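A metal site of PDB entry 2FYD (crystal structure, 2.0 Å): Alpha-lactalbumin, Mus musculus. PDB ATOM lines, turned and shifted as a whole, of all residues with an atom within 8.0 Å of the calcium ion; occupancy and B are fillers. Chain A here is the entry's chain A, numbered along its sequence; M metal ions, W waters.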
ATOM      1  N   THR A  38      -9.670 -19.905 -18.793  1.00  0.00           N
ATOM      2  CA  THR A  38      -8.714 -20.564 -17.911  1.00  0.00           C
ATOM      3  C   THR A  38      -8.233 -21.927 -18.414  1.00  0.00           C
ATOM      4  O   THR A  38      -7.277 -22.472 -17.868  1.00  0.00           O
ATOM      5  CB  THR A  38      -9.302 -20.724 -16.479  1.00  0.00           C
ATOM      6  OG1 THR A  38     -10.382 -21.664 -16.490  1.00  0.00           O
ATOM      7  CG2 THR A  38      -9.826 -19.393 -15.992  1.00  0.00           C
ATOM      8  N   ILE A  75       6.278 -25.826 -11.375  1.00  0.00           N
ATOM      9  CA  ILE A  75       4.915 -26.297 -11.325  1.00  0.00           C
ATOM     10  C   ILE A  75       4.551 -27.037 -12.607  1.00  0.00           C
ATOM     11  O   ILE A  75       5.151 -26.811 -13.658  1.00  0.00           O
ATOM     12  CB  ILE A  75       3.965 -25.086 -11.066  1.00  0.00           C
ATOM     13  CG1 ILE A  75       2.544 -25.573 -10.782  1.00  0.00           C
ATOM     14  CG2 ILE A  75       3.955 -24.156 -12.247  1.00  0.00           C
ATOM     15  CD1 ILE A  75       1.589 -24.450 -10.660  1.00  0.00           C
ATOM     16  N   SER A  76       3.614 -27.968 -12.508  1.00  0.00           N
ATOM     17  CA  SER A  76       3.132 -28.725 -13.656  1.00  0.00           C
ATOM     18  C   SER A  76       2.244 -27.774 -14.466  1.00  0.00           C
ATOM     19  O   SER A  76       1.474 -27.002 -13.873  1.00  0.00           O
ATOM     20  CB  SER A  76       2.303 -29.935 -13.183  1.00  0.00           C
ATOM     21  OG  SER A  76       1.433 -30.420 -14.203  1.00  0.00           O
ATOM     22  N   CYS A  77       2.321 -27.832 -15.783  1.00  0.00           N
ATOM     23  CA  CYS A  77       1.479 -26.935 -16.592  1.00  0.00           C
ATOM     24  C   CYS A  77      -0.023 -27.222 -16.416  1.00  0.00           C
ATOM     25  O   CYS A  77      -0.868 -26.333 -16.641  1.00  0.00           O
ATOM     26  CB  CYS A  77       1.857 -27.036 -18.062  1.00  0.00           C
ATOM     27  SG  CYS A  77       3.609 -26.728 -18.496  1.00  0.00           S
ATOM     28  N   ASP A  78      -0.378 -28.449 -16.004  1.00  0.00           N
ATOM     29  CA  ASP A  78      -1.804 -28.793 -15.803  1.00  0.00           C
ATOM     30  C   ASP A  78      -2.441 -27.970 -14.691  1.00  0.00           C
ATOM     31  O   ASP A  78      -3.656 -27.796 -14.693  1.00  0.00           O
ATOM     32  CB  ASP A  78      -2.009 -30.278 -15.485  1.00  0.00           C
ATOM     33  CG  ASP A  78      -1.687 -31.172 -16.683  1.00  0.00           C
ATOM     34  OD1 ASP A  78      -1.911 -30.728 -17.830  1.00  0.00           O
ATOM     35  OD2 ASP A  78      -1.223 -32.311 -16.464  1.00  0.00           O
ATOM     36  N   LYS A  79      -1.632 -27.495 -13.734  1.00  0.00           N
ATOM     37  CA  LYS A  79      -2.118 -26.657 -12.620  1.00  0.00           C
ATOM     38  C   LYS A  79      -2.533 -25.271 -13.118  1.00  0.00           C
ATOM     39  O   LYS A  79      -3.092 -24.428 -12.352  1.00  0.00           O
ATOM     40  CB  LYS A  79      -1.041 -26.463 -11.546  1.00  0.00           C
ATOM     41  CG  LYS A  79      -0.743 -27.683 -10.629  1.00  0.00           C
ATOM     42  CD  LYS A  79      -1.948 -27.997  -9.722  1.00  0.00           C
ATOM     43  CE  LYS A  79      -1.596 -29.091  -8.723  1.00  0.00           C
ATOM     44  NZ  LYS A  79      -2.807 -29.440  -7.903  1.00  0.00           N
ATOM     45  N   LEU A  80      -2.235 -25.011 -14.389  1.00  0.00           N
ATOM     46  CA  LEU A  80      -2.522 -23.719 -15.007  1.00  0.00           C
ATOM     47  C   LEU A  80      -3.794 -23.770 -15.872  1.00  0.00           C
ATOM     48  O   LEU A  80      -4.134 -22.784 -16.552  1.00  0.00           O
ATOM     49  CB  LEU A  80      -1.322 -23.248 -15.855  1.00  0.00           C
ATOM     50  CG  LEU A  80       0.007 -23.061 -15.085  1.00  0.00           C
ATOM     51  CD1 LEU A  80       1.163 -22.701 -16.046  1.00  0.00           C
ATOM     52  CD2 LEU A  80      -0.174 -21.990 -14.019  1.00  0.00           C
ATOM     53  N   LEU A  81      -4.487 -24.908 -15.855  1.00  0.00           N
ATOM     54  CA  LEU A  81      -5.723 -25.057 -16.608  1.00  0.00           C
ATOM     55  C   LEU A  81      -6.967 -25.204 -15.710  1.00  0.00           C
ATOM     56  O   LEU A  81      -7.971 -25.781 -16.120  1.00  0.00           O
ATOM     57  CB  LEU A  81      -5.620 -26.265 -17.570  1.00  0.00           C
ATOM     58  CG  LEU A  81      -4.418 -26.212 -18.542  1.00  0.00           C
ATOM     59  CD1 LEU A  81      -4.298 -27.537 -19.334  1.00  0.00           C
ATOM     60  CD2 LEU A  81      -4.625 -25.044 -19.513  1.00  0.00           C
ATOM     61  N   ASP A  82      -6.933 -24.698 -14.484  1.00  0.00           N
ATOM     62  CA  ASP A  82      -8.113 -24.782 -13.612  1.00  0.00           C
ATOM     63  C   ASP A  82      -8.586 -23.378 -13.229  1.00  0.00           C
ATOM     64  O   ASP A  82      -7.993 -22.394 -13.684  1.00  0.00           O
ATOM     65  CB  ASP A  82      -7.811 -25.633 -12.351  1.00  0.00           C
ATOM     66  CG  ASP A  82      -6.590 -25.157 -11.583  1.00  0.00           C
ATOM     67  OD1 ASP A  82      -6.456 -23.947 -11.388  1.00  0.00           O
ATOM     68  OD2 ASP A  82      -5.758 -26.000 -11.165  1.00  0.00           O
ATOM     69  N   ASP A  83      -9.626 -23.278 -12.400  1.00  0.00           N
ATOM     70  CA  ASP A  83     -10.166 -21.975 -11.988  1.00  0.00           C
ATOM     71  C   ASP A  83      -9.540 -21.376 -10.717  1.00  0.00           C
ATOM     72  O   ASP A  83     -10.026 -20.386 -10.180  1.00  0.00           O
ATOM     73  CB  ASP A  83     -11.693 -22.076 -11.822  1.00  0.00           C
ATOM     74  CG  ASP A  83     -12.413 -22.322 -13.158  1.00  0.00           C
ATOM     75  OD1 ASP A  83     -11.764 -22.246 -14.233  1.00  0.00           O
ATOM     76  OD2 ASP A  83     -13.629 -22.579 -13.131  1.00  0.00           O
ATOM     77  N   GLU A  84      -8.431 -21.938 -10.261  1.00  0.00           N
ATOM     78  CA  GLU A  84      -7.726 -21.438  -9.065  1.00  0.00           C
ATOM     79  C   GLU A  84      -6.461 -20.724  -9.572  1.00  0.00           C
ATOM     80  O   GLU A  84      -5.454 -21.331  -9.922  1.00  0.00           O
ATOM     81  CB  GLU A  84      -7.419 -22.615  -8.133  1.00  0.00           C
ATOM     82  CG  GLU A  84      -8.718 -23.222  -7.537  1.00  0.00           C
ATOM     83  CD  GLU A  84      -8.520 -24.652  -7.004  1.00  0.00           C
ATOM     84  OE1 GLU A  84      -7.628 -24.864  -6.153  1.00  0.00           O
ATOM     85  OE2 GLU A  84      -9.253 -25.547  -7.455  1.00  0.00           O
ATOM     86  N   LEU A  85      -6.568 -19.394  -9.606  1.00  0.00           N
ATOM     87  CA  LEU A  85      -5.554 -18.501 -10.153  1.00  0.00           C
ATOM     88  C   LEU A  85      -4.361 -18.118  -9.285  1.00  0.00           C
ATOM     89  O   LEU A  85      -3.436 -17.472  -9.788  1.00  0.00           O
ATOM     90  CB  LEU A  85      -6.280 -17.236 -10.653  1.00  0.00           C
ATOM     91  CG  LEU A  85      -6.798 -17.192 -12.106  1.00  0.00           C
ATOM     92  CD1 LEU A  85      -6.761 -18.546 -12.740  1.00  0.00           C
ATOM     93  CD2 LEU A  85      -8.178 -16.582 -12.186  1.00  0.00           C
ATOM     94  N   ASP A  86      -4.342 -18.519  -8.024  1.00  0.00           N
ATOM     95  CA  ASP A  86      -3.218 -18.171  -7.172  1.00  0.00           C
ATOM     96  C   ASP A  86      -1.881 -18.663  -7.731  1.00  0.00           C
ATOM     97  O   ASP A  86      -0.914 -17.889  -7.785  1.00  0.00           O
ATOM     98  CB  ASP A  86      -3.386 -18.727  -5.745  1.00  0.00           C
ATOM     99  CG  ASP A  86      -4.566 -18.113  -4.987  1.00  0.00           C
ATOM    100  OD1 ASP A  86      -5.715 -18.410  -5.359  1.00  0.00           O
ATOM    101  OD2 ASP A  86      -4.346 -17.342  -4.033  1.00  0.00           O
ATOM    102  N   ASP A  87      -1.803 -19.923  -8.165  1.00  0.00           N
ATOM    103  CA  ASP A  87      -0.512 -20.391  -8.645  1.00  0.00           C
ATOM    104  C   ASP A  87      -0.151 -19.775 -10.023  1.00  0.00           C
ATOM    105  O   ASP A  87       1.029 -19.539 -10.279  1.00  0.00           O
ATOM    106  CB  ASP A  87      -0.409 -21.927  -8.604  1.00  0.00           C
ATOM    107  CG  ASP A  87      -1.584 -22.664  -9.274  1.00  0.00           C
ATOM    108  OD1 ASP A  87      -2.463 -22.030  -9.929  1.00  0.00           O
ATOM    109  OD2 ASP A  87      -1.627 -23.915  -9.128  1.00  0.00           O
ATOM    110  N   ASP A  88      -1.156 -19.505 -10.872  1.00  0.00           N
ATOM    111  CA  ASP A  88      -0.926 -18.874 -12.191  1.00  0.00           C
ATOM    112  C   ASP A  88      -0.321 -17.483 -11.956  1.00  0.00           C
ATOM    113  O   ASP A  88       0.633 -17.086 -12.632  1.00  0.00           O
ATOM    114  CB  ASP A  88      -2.249 -18.664 -12.992  1.00  0.00           C
ATOM    115  CG  ASP A  88      -2.997 -19.958 -13.237  1.00  0.00           C
ATOM    116  OD1 ASP A  88      -3.396 -20.230 -14.400  1.00  0.00           O
ATOM    117  OD2 ASP A  88      -3.166 -20.699 -12.245  1.00  0.00           O
ATOM    118  N   ILE A  89      -0.902 -16.748 -11.028  1.00  0.00           N
ATOM    119  CA  ILE A  89      -0.431 -15.401 -10.711  1.00  0.00           C
ATOM    120  C   ILE A  89       1.010 -15.437 -10.169  1.00  0.00           C
ATOM    121  O   ILE A  89       1.838 -14.605 -10.563  1.00  0.00           O
ATOM    122  CB  ILE A  89      -1.381 -14.709  -9.699  1.00  0.00           C
ATOM    123  CG1 ILE A  89      -2.745 -14.478 -10.354  1.00  0.00           C
ATOM    124  CG2 ILE A  89      -0.771 -13.387  -9.202  1.00  0.00           C
ATOM    125  CD1 ILE A  89      -3.912 -14.240  -9.341  1.00  0.00           C
HETATM  126 CA    CA M   1      -4.312 -22.654 -11.343  1.00  0.00          CA
HETATM  127  O   HOH W   1      -5.344 -22.282 -13.650  1.00  0.00           O
HETATM  128  O   HOH W   2      -4.322 -24.389  -9.503  1.00  0.00           O
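Five residues have an atom within 4 Å of the calcium ion: Lys 79, Asp 82, Glu 84, Asp 87 and Asp 88.
The nearest printed residue that does not touch the calcium ion is Leu 80 (4.2 Å).
The calcium ion is bound by O of Glu 84 (2.3 Å).
O of Lys 79 is bound to the calcium ion (2.4 Å).
The side-chain carboxylate (OD1) of Asp 87 is bound to the calcium ion (2.4 Å).
The calcium ion is bound by the side-chain carboxylate (OD2) of Asp 88 (2.4 Å).
OD1 of Asp 82 binds the calcium ion, at 2.5 Å.
Water W2 binds the calcium ion (2.5 Å).
The calcium ion is bound by water W1.
The calcium ion has seven donor atoms within binding distance.
Water W2 bridges the side-chain carboxylate of Asp 82 (2.7 Å) and the side-chain carboxylate of Asp 87 (2.8 Å).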
